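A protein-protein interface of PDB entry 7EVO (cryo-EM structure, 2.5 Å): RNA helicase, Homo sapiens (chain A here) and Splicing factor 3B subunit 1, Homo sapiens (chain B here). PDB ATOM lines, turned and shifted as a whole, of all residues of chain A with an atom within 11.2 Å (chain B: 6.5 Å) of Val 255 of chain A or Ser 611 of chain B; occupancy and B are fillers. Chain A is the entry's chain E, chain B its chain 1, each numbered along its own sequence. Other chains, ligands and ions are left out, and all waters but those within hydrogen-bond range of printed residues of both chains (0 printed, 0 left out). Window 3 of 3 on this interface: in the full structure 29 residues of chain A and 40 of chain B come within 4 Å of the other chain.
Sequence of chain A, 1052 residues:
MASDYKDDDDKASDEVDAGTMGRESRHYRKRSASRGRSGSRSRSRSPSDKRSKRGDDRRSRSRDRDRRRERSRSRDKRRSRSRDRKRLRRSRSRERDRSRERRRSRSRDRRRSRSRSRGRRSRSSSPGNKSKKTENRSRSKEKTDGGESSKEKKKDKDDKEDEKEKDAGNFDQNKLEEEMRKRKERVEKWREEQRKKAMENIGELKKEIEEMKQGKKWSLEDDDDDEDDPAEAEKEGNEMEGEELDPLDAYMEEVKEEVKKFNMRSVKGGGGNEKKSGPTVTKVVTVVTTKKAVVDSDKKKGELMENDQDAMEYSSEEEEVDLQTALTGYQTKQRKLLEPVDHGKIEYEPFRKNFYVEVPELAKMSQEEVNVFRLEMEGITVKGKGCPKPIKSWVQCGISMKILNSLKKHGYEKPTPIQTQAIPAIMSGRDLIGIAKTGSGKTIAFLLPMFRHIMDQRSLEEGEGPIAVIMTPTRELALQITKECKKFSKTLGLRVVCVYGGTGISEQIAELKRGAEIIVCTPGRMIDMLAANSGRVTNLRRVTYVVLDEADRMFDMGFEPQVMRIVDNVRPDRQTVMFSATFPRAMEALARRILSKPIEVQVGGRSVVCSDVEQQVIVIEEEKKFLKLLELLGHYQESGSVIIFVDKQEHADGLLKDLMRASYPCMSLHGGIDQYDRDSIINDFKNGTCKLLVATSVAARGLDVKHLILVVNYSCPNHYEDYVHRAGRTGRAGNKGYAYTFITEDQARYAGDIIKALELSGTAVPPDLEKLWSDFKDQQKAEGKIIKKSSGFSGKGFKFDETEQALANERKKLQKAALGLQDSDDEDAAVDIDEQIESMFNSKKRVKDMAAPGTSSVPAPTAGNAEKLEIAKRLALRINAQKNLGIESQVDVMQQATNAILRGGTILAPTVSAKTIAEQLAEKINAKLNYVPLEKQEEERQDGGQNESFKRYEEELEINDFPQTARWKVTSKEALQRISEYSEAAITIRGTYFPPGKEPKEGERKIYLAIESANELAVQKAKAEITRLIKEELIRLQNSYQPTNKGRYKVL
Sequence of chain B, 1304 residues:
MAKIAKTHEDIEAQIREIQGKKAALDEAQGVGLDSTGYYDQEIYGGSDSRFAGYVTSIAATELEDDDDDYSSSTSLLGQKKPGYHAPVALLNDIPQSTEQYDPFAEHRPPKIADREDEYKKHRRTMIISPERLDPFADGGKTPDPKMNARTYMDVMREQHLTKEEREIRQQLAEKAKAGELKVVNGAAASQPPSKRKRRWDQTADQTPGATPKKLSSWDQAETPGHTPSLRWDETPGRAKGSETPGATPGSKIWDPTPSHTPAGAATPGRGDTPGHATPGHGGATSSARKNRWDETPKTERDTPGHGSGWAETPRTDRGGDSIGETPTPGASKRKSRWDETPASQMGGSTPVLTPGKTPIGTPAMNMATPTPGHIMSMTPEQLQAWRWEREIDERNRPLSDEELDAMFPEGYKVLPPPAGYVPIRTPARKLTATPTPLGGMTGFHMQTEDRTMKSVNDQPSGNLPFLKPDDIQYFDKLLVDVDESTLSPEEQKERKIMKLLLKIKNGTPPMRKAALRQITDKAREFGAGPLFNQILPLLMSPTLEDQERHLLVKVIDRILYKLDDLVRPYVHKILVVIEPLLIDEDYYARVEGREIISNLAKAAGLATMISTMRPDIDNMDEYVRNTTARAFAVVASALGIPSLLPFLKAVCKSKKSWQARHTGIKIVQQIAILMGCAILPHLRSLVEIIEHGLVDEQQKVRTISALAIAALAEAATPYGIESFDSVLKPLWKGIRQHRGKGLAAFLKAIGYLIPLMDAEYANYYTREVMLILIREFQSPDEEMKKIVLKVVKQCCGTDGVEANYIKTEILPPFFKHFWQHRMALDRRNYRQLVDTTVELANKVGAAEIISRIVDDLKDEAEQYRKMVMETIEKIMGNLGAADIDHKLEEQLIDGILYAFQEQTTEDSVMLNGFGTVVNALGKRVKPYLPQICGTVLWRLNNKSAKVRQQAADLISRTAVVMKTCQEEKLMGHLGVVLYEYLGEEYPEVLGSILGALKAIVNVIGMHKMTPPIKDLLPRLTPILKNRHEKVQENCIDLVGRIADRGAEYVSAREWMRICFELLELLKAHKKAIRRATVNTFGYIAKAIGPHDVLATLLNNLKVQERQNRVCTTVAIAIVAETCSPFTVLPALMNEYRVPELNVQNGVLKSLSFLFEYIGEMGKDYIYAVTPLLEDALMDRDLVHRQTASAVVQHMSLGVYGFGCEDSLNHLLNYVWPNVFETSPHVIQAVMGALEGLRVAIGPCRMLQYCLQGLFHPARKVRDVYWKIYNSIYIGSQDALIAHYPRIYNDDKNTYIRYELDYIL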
ATOM      1  N   PRO A 247      18.601  11.227  27.471  1.00  0.00           N
ATOM      2  CA  PRO A 247      18.576  12.084  26.285  1.00  0.00           C
ATOM      3  C   PRO A 247      18.978  11.307  25.025  1.00  0.00           C
ATOM      4  O   PRO A 247      18.644  11.742  23.939  1.00  0.00           O
ATOM      5  CB  PRO A 247      19.653  13.125  26.614  1.00  0.00           C
ATOM      6  CG  PRO A 247      20.667  12.348  27.423  1.00  0.00           C
ATOM      7  CD  PRO A 247      19.849  11.360  28.229  1.00  0.00           C
ATOM      8  N   LEU A 248      19.676  10.181  25.205  1.00  0.00           N
ATOM      9  CA  LEU A 248      20.144   9.350  24.064  1.00  0.00           C
ATOM     10  C   LEU A 248      18.979   8.528  23.502  1.00  0.00           C
ATOM     11  O   LEU A 248      18.872   8.432  22.264  1.00  0.00           O
ATOM     12  CB  LEU A 248      21.282   8.440  24.535  1.00  0.00           C
ATOM     13  CG  LEU A 248      22.290   8.042  23.458  1.00  0.00           C
ATOM     14  CD1 LEU A 248      22.859   6.659  23.728  1.00  0.00           C
ATOM     15  CD2 LEU A 248      21.657   8.098  22.077  1.00  0.00           C
ATOM     16  N   ASP A 249      18.142   7.960  24.376  1.00  0.00           N
ATOM     17  CA  ASP A 249      17.002   7.128  23.909  1.00  0.00           C
ATOM     18  C   ASP A 249      15.934   8.040  23.299  1.00  0.00           C
ATOM     19  O   ASP A 249      15.402   7.684  22.233  1.00  0.00           O
ATOM     20  CB  ASP A 249      16.427   6.298  25.058  1.00  0.00           C
ATOM     21  CG  ASP A 249      17.478   5.470  25.774  1.00  0.00           C
ATOM     22  OD1 ASP A 249      18.536   6.035  26.115  1.00  0.00           O
ATOM     23  OD2 ASP A 249      17.232   4.266  25.981  1.00  0.00           O
ATOM     24  N   ALA A 250      15.668   9.188  23.931  1.00  0.00           N
ATOM     25  CA  ALA A 250      14.664  10.157  23.426  1.00  0.00           C
ATOM     26  C   ALA A 250      15.009  10.561  21.988  1.00  0.00           C
ATOM     27  O   ALA A 250      14.117  10.483  21.118  1.00  0.00           O
ATOM     28  CB  ALA A 250      14.612  11.357  24.337  1.00  0.00           C
ATOM     29  N   TYR A 251      16.259  10.973  21.751  1.00  0.00           N
ATOM     30  CA  TYR A 251      16.718  11.361  20.389  1.00  0.00           C
ATOM     31  C   TYR A 251      16.640  10.139  19.469  1.00  0.00           C
ATOM     32  O   TYR A 251      16.234  10.278  18.296  1.00  0.00           O
ATOM     33  CB  TYR A 251      18.150  11.902  20.429  1.00  0.00           C
ATOM     34  CG  TYR A 251      18.692  12.291  19.078  1.00  0.00           C
ATOM     35  CD1 TYR A 251      19.401  11.389  18.304  1.00  0.00           C
ATOM     36  CD2 TYR A 251      18.479  13.556  18.561  1.00  0.00           C
ATOM     37  CE1 TYR A 251      19.892  11.735  17.057  1.00  0.00           C
ATOM     38  CE2 TYR A 251      18.964  13.921  17.317  1.00  0.00           C
ATOM     39  CZ  TYR A 251      19.672  13.007  16.560  1.00  0.00           C
ATOM     40  OH  TYR A 251      20.153  13.359  15.335  1.00  0.00           O
ATOM     41  N   MET A 252      17.010   8.973  20.002  1.00  0.00           N
ATOM     42  CA  MET A 252      16.955   7.720  19.208  1.00  0.00           C
ATOM     43  C   MET A 252      15.495   7.467  18.833  1.00  0.00           C
ATOM     44  O   MET A 252      15.230   7.157  17.659  1.00  0.00           O
ATOM     45  CB  MET A 252      17.480   6.537  20.025  1.00  0.00           C
ATOM     46  CG  MET A 252      18.325   5.595  19.202  1.00  0.00           C
ATOM     47  SD  MET A 252      19.594   6.511  18.303  1.00  0.00           S
ATOM     48  CE  MET A 252      19.727   5.510  16.824  1.00  0.00           C
ATOM     49  N   GLU A 253      14.587   7.643  19.797  1.00  0.00           N
ATOM     50  CA  GLU A 253      13.136   7.426  19.548  1.00  0.00           C
ATOM     51  C   GLU A 253      12.679   8.383  18.443  1.00  0.00           C
ATOM     52  O   GLU A 253      11.920   7.945  17.563  1.00  0.00           O
ATOM     53  CB  GLU A 253      12.336   7.666  20.829  1.00  0.00           C
ATOM     54  CG  GLU A 253      12.429   6.524  21.825  1.00  0.00           C
ATOM     55  CD  GLU A 253      11.763   6.800  23.162  1.00  0.00           C
ATOM     56  OE1 GLU A 253      11.141   7.872  23.299  1.00  0.00           O
ATOM     57  OE2 GLU A 253      11.867   5.942  24.063  1.00  0.00           O
ATOM     58  N   GLU A 254      13.151   9.632  18.475  1.00  0.00           N
ATOM     59  CA  GLU A 254      12.786  10.625  17.429  1.00  0.00           C
ATOM     60  C   GLU A 254      13.290  10.140  16.063  1.00  0.00           C
ATOM     61  O   GLU A 254      12.530  10.258  15.087  1.00  0.00           O
ATOM     62  CB  GLU A 254      13.411  11.983  17.747  1.00  0.00           C
ATOM     63  CG  GLU A 254      13.278  12.982  16.613  1.00  0.00           C
ATOM     64  CD  GLU A 254      14.243  14.152  16.689  1.00  0.00           C
ATOM     65  OE1 GLU A 254      13.822  15.286  16.391  1.00  0.00           O
ATOM     66  OE2 GLU A 254      15.415  13.925  17.042  1.00  0.00           O
ATOM     67  N   VAL A 255      14.513   9.599  16.008  1.00  0.00           N
ATOM     68  CA  VAL A 255      15.091   9.079  14.728  1.00  0.00           C
ATOM     69  C   VAL A 255      14.272   7.871  14.253  1.00  0.00           C
ATOM     70  O   VAL A 255      13.796   7.903  13.101  1.00  0.00           O
ATOM     71  CB  VAL A 255      16.583   8.719  14.878  1.00  0.00           C
ATOM     72  CG1 VAL A 255      17.018   7.672  13.867  1.00  0.00           C
ATOM     73  CG2 VAL A 255      17.470   9.951  14.787  1.00  0.00           C
ATOM     74  N   LYS A 256      14.132   6.853  15.111  1.00  0.00           N
ATOM     75  CA  LYS A 256      13.361   5.614  14.822  1.00  0.00           C
ATOM     76  C   LYS A 256      12.010   6.009  14.221  1.00  0.00           C
ATOM     77  O   LYS A 256      11.586   5.373  13.236  1.00  0.00           O
ATOM     78  CB  LYS A 256      13.177   4.791  16.101  1.00  0.00           C
ATOM     79  CG  LYS A 256      14.444   4.139  16.640  1.00  0.00           C
ATOM     80  CD  LYS A 256      15.203   3.354  15.591  1.00  0.00           C
ATOM     81  CE  LYS A 256      16.560   2.880  16.066  1.00  0.00           C
ATOM     82  NZ  LYS A 256      17.270   2.114  15.015  1.00  0.00           N
ATOM     83  N   GLU A 257      11.388   7.052  14.778  1.00  0.00           N
ATOM     84  CA  GLU A 257      10.079   7.548  14.280  1.00  0.00           C
ATOM     85  C   GLU A 257      10.243   8.014  12.831  1.00  0.00           C
ATOM     86  O   GLU A 257       9.375   7.677  12.003  1.00  0.00           O
ATOM     87  CB  GLU A 257       9.578   8.696  15.158  1.00  0.00           C
ATOM     88  CG  GLU A 257       8.880   8.231  16.423  1.00  0.00           C
ATOM     89  CD  GLU A 257       8.333   9.352  17.289  1.00  0.00           C
ATOM     90  OE1 GLU A 257       8.476  10.526  16.892  1.00  0.00           O
ATOM     91  OE2 GLU A 257       7.766   9.049  18.357  1.00  0.00           O
ATOM     92  N   GLU A 258      11.335   8.728  12.532  1.00  0.00           N
ATOM     93  CA  GLU A 258      11.544   9.234  11.149  1.00  0.00           C
ATOM     94  C   GLU A 258      11.732   8.046  10.198  1.00  0.00           C
ATOM     95  O   GLU A 258      11.044   8.004   9.151  1.00  0.00           O
ATOM     96  CB  GLU A 258      12.754  10.158  11.122  1.00  0.00           C
ATOM     97  CG  GLU A 258      13.106  10.673   9.741  1.00  0.00           C
ATOM     98  CD  GLU A 258      14.151  11.777   9.749  1.00  0.00           C
ATOM     99  OE1 GLU A 258      14.688  12.089  10.835  1.00  0.00           O
ATOM    100  OE2 GLU A 258      14.433  12.324   8.665  1.00  0.00           O
ATOM    101  N   VAL A 259      12.583   7.086  10.568  1.00  0.00           N
ATOM    102  CA  VAL A 259      12.866   5.915   9.682  1.00  0.00           C
ATOM    103  C   VAL A 259      11.572   5.120   9.470  1.00  0.00           C
ATOM    104  O   VAL A 259      11.280   4.758   8.306  1.00  0.00           O
ATOM    105  CB  VAL A 259      13.993   5.032  10.244  1.00  0.00           C
ATOM    106  CG1 VAL A 259      13.818   3.577   9.854  1.00  0.00           C
ATOM    107  CG2 VAL A 259      15.364   5.534   9.814  1.00  0.00           C
ATOM    108  N   LYS A 260      10.810   4.879  10.537  1.00  0.00           N
ATOM    109  CA  LYS A 260       9.560   4.082  10.420  1.00  0.00           C
ATOM    110  C   LYS A 260       8.596   4.806   9.476  1.00  0.00           C
ATOM    111  O   LYS A 260       8.000   4.126   8.615  1.00  0.00           O
ATOM    112  CB  LYS A 260       8.900   3.870  11.781  1.00  0.00           C
ATOM    113  CG  LYS A 260       7.572   3.123  11.738  1.00  0.00           C
ATOM    114  CD  LYS A 260       6.842   3.064  13.055  1.00  0.00           C
ATOM    115  CE  LYS A 260       5.498   2.375  12.947  1.00  0.00           C
ATOM    116  NZ  LYS A 260       4.856   2.191  14.275  1.00  0.00           N
ATOM    117  N   LYS A 261       8.481   6.129   9.617  1.00  0.00           N
ATOM    118  CA  LYS A 261       7.555   6.931   8.782  1.00  0.00           C
ATOM    119  C   LYS A 261       7.999   6.805   7.324  1.00  0.00           C
ATOM    120  O   LYS A 261       7.146   6.596   6.453  1.00  0.00           O
ATOM    121  CB  LYS A 261       7.551   8.396   9.227  1.00  0.00           C
ATOM    122  CG  LYS A 261       6.230   9.125   9.027  1.00  0.00           C
ATOM    123  CD  LYS A 261       5.545   8.864   7.697  1.00  0.00           C
ATOM    124  CE  LYS A 261       4.815   7.544   7.609  1.00  0.00           C
ATOM    125  NZ  LYS A 261       3.762   7.430   8.644  1.00  0.00           N
ATOM    126  N   PHE A 262       9.292   6.916   7.054  1.00  0.00           N
ATOM    127  CA  PHE A 262       9.772   6.831   5.653  1.00  0.00           C
ATOM    128  C   PHE A 262       9.423   5.448   5.097  1.00  0.00           C
ATOM    129  O   PHE A 262       8.943   5.365   3.943  1.00  0.00           O
ATOM    130  CB  PHE A 262      11.272   7.085   5.538  1.00  0.00           C
ATOM    131  CG  PHE A 262      11.822   6.718   4.188  1.00  0.00           C
ATOM    132  CD1 PHE A 262      12.672   5.629   4.035  1.00  0.00           C
ATOM    133  CD2 PHE A 262      11.456   7.437   3.061  1.00  0.00           C
ATOM    134  CE1 PHE A 262      13.138   5.266   2.780  1.00  0.00           C
ATOM    135  CE2 PHE A 262      11.949   7.090   1.808  1.00  0.00           C
ATOM    136  CZ  PHE A 262      12.784   6.002   1.669  1.00  0.00           C
ATOM    137  N   ASN A 263       9.638   4.397   5.898  1.00  0.00           N
ATOM    138  CA  ASN A 263       9.324   3.008   5.464  1.00  0.00           C
ATOM    139  C   ASN A 263       7.805   2.827   5.385  1.00  0.00           C
ATOM    140  O   ASN A 263       7.292   2.584   4.293  1.00  0.00           O
ATOM    141  CB  ASN A 263       9.977   1.964   6.368  1.00  0.00           C
ATOM    142  CG  ASN A 263      11.349   1.541   5.884  1.00  0.00           C
ATOM    143  OD1 ASN A 263      12.319   1.572   6.641  1.00  0.00           O
ATOM    144  ND2 ASN A 263      11.441   1.145   4.625  1.00  0.00           N
ATOM    145  N   LEU B 606      21.285  10.393   6.941  1.00  0.00           N
ATOM    146  CA  LEU B 606      21.899  10.469   8.263  1.00  0.00           C
ATOM    147  C   LEU B 606      21.184   9.560   9.256  1.00  0.00           C
ATOM    148  O   LEU B 606      21.829   8.887  10.072  1.00  0.00           O
ATOM    149  CB  LEU B 606      21.894  11.918   8.751  1.00  0.00           C
ATOM    150  CG  LEU B 606      22.491  12.219  10.125  1.00  0.00           C
ATOM    151  CD1 LEU B 606      23.484  13.356  10.022  1.00  0.00           C
ATOM    152  CD2 LEU B 606      21.389  12.569  11.108  1.00  0.00           C
ATOM    153  N   ALA B 607      19.850   9.526   9.199  1.00  0.00           N
ATOM    154  CA  ALA B 607      19.084   8.715  10.139  1.00  0.00           C
ATOM    155  C   ALA B 607      19.398   7.234   9.979  1.00  0.00           C
ATOM    156  O   ALA B 607      19.501   6.506  10.971  1.00  0.00           O
ATOM    157  CB  ALA B 607      17.590   8.971   9.955  1.00  0.00           C
ATOM    158  N   THR B 608      19.567   6.772   8.738  1.00  0.00           N
ATOM    159  CA  THR B 608      19.883   5.365   8.506  1.00  0.00           C
ATOM    160  C   THR B 608      21.249   5.007   9.082  1.00  0.00           C
ATOM    161  O   THR B 608      21.395   3.995   9.781  1.00  0.00           O
ATOM    162  CB  THR B 608      19.835   5.059   7.009  1.00  0.00           C
ATOM    163  OG1 THR B 608      18.491   5.195   6.537  1.00  0.00           O
ATOM    164  CG2 THR B 608      20.324   3.644   6.733  1.00  0.00           C
ATOM    165  N   MET B 609      22.262   5.829   8.796  1.00  0.00           N
ATOM    166  CA  MET B 609      23.596   5.576   9.329  1.00  0.00           C
ATOM    167  C   MET B 609      23.579   5.558  10.850  1.00  0.00           C
ATOM    168  O   MET B 609      24.175   4.676  11.478  1.00  0.00           O
ATOM    169  CB  MET B 609      24.577   6.630   8.813  1.00  0.00           C
ATOM    170  CG  MET B 609      24.685   6.704   7.300  1.00  0.00           C
ATOM    171  SD  MET B 609      25.212   5.154   6.551  1.00  0.00           S
ATOM    172  CE  MET B 609      26.973   5.207   6.865  1.00  0.00           C
ATOM    173  N   ILE B 610      22.881   6.519  11.460  1.00  0.00           N
ATOM    174  CA  ILE B 610      22.820   6.569  12.918  1.00  0.00           C
ATOM    175  C   ILE B 610      22.108   5.341  13.468  1.00  0.00           C
ATOM    176  O   ILE B 610      22.530   4.761  14.474  1.00  0.00           O
ATOM    177  CB  ILE B 610      22.147   7.876  13.379  1.00  0.00           C
ATOM    178  CG1 ILE B 610      23.103   9.055  13.199  1.00  0.00           C
ATOM    179  CG2 ILE B 610      21.700   7.773  14.830  1.00  0.00           C
ATOM    180  CD1 ILE B 610      22.548  10.362  13.697  1.00  0.00           C
ATOM    181  N   SER B 611      21.036   4.902  12.801  1.00  0.00           N
ATOM    182  CA  SER B 611      20.251   3.788  13.321  1.00  0.00           C
ATOM    183  C   SER B 611      21.006   2.470  13.209  1.00  0.00           C
ATOM    184  O   SER B 611      20.823   1.573  14.040  1.00  0.00           O
ATOM    185  CB  SER B 611      18.913   3.706  12.588  1.00  0.00           C
ATOM    186  OG  SER B 611      18.274   4.969  12.552  1.00  0.00           O
ATOM    187  N   THR B 612      21.854   2.327  12.188  1.00  0.00           N
ATOM    188  CA  THR B 612      22.635   1.096  12.076  1.00  0.00           C
ATOM    189  C   THR B 612      23.890   1.146  12.944  1.00  0.00           C
ATOM    190  O   THR B 612      24.388   0.103  13.386  1.00  0.00           O
ATOM    191  CB  THR B 612      23.001   0.806  10.619  1.00  0.00           C
ATOM    192  OG1 THR B 612      24.092   1.640  10.211  1.00  0.00           O
ATOM    193  CG2 THR B 612      21.806   0.996   9.700  1.00  0.00           C
ATOM    194  N   MET B 613      24.418   2.342  13.206  1.00  0.00           N
ATOM    195  CA  MET B 613      25.655   2.462  13.968  1.00  0.00           C
ATOM    196  C   MET B 613      25.440   2.614  15.470  1.00  0.00           C
ATOM    197  O   MET B 613      26.397   2.451  16.232  1.00  0.00           O
ATOM    198  CB  MET B 613      26.472   3.651  13.455  1.00  0.00           C
ATOM    199  CG  MET B 613      27.200   3.396  12.149  1.00  0.00           C
ATOM    200  SD  MET B 613      27.991   4.887  11.519  1.00  0.00           S
ATOM    201  CE  MET B 613      28.900   4.223  10.129  1.00  0.00           C
ATOM    202  N   ARG B 614      24.222   2.923  15.916  1.00  0.00           N
ATOM    203  CA  ARG B 614      23.956   3.151  17.333  1.00  0.00           C
ATOM    204  C   ARG B 614      24.062   1.902  18.209  1.00  0.00           C
ATOM    205  O   ARG B 614      24.514   2.014  19.354  1.00  0.00           O
ATOM    206  CB  ARG B 614      22.570   3.779  17.507  1.00  0.00           C
ATOM    207  CG  ARG B 614      22.352   4.432  18.864  1.00  0.00           C
ATOM    208  CD  ARG B 614      21.509   3.558  19.778  1.00  0.00           C
ATOM    209  NE  ARG B 614      21.606   3.972  21.174  1.00  0.00           N
ATOM    210  CZ  ARG B 614      22.431   3.424  22.060  1.00  0.00           C
ATOM    211  NH1 ARG B 614      23.233   2.433  21.696  1.00  0.00           N
ATOM    212  NH2 ARG B 614      22.453   3.863  23.310  1.00  0.00           N
ATOM    213  N   PRO B 615      23.646   0.710  17.753  1.00  0.00           N
ATOM    214  CA  PRO B 615      23.769  -0.461  18.642  1.00  0.00           C
ATOM    215  C   PRO B 615      25.202  -0.794  19.021  1.00  0.00           C
ATOM    216  O   PRO B 615      25.440  -1.295  20.126  1.00  0.00           O
ATOM    217  CB  PRO B 615      23.117  -1.594  17.832  1.00  0.00           C
ATOM    218  CG  PRO B 615      23.011  -1.087  16.440  1.00  0.00           C
ATOM    219  CD  PRO B 615      22.847   0.386  16.559  1.00  0.00           C
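The side-chain hydroxyl (OG) of Ser 611 of chain B is in hydrogen-bond range of the backbone carbonyl oxygen (O) of Ala 607 of chain B.
Arg 614 of chain B touches Leu 248 of chain A. Ile 610 of chain B touches Met 252 of chain A (CG2 to CE, 3.6 Å). Met 252 of chain A touches Ser 611 of chain B (CE to CA, 3.9 Å). Arg 614 of chain B touches Met 252 of chain A (CB to CE, 3.4 Å). Val 255 of chain A touches Ala 607 of chain B. CG1 of Val 255 of chain A touches OG of Ser 611 of chain B (3.3 Å). NZ of Lys 256 of chain A touches CB of Ser 611 of chain B, at 3.3 Å.
Printed residues of chain B within 4 Å of Leu 248 of chain A: Arg 614. Printed residues of chain B within 4 Å of Met 252 of chain A: Ile 610 (3.6 Å), Ser 611 (3.9 Å) and Arg 614 (3.4 Å). Printed residues of chain B within 4 Å of Val 255 of chain A: Ala 607 (3.99 Å) and Ser 611 (3.3 Å). Of the printed residues of chain B, Lys 256 of chain A touches Ser 611 (3.3 Å). Of the printed residues of chain A, Ala 607 of chain B touches Val 255. No residue of chain A comes within 4 Å of Thr 608 of chain B. Of chain A, only Met 252 comes within 4 Å of Ile 610 of chain B. No residue of chain A comes within 4 Å of Thr 612 of chain B. Printed residues of chain A within 4 Å of Arg 614 of chain B: Leu 248 and Met 252. The nearest printed residue of chain B that does not touch Val 255 of chain A is Ile 610 of chain B (4.8 Å). The nearest residue of chain A that does not touch Ser 611 of chain B is Val 259 of chain A (4.04 Å).
Hydrophobic or aromatic side chains of chain A that line the printed part of chain B: Leu 248, Met 252 and Val 255. Printed residues of chain B that touch a printed residue of chain A: Ala 607, Ile 610, Ser 611 and Arg 614. Among the printed residues, 7 pairs touch across the chains.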
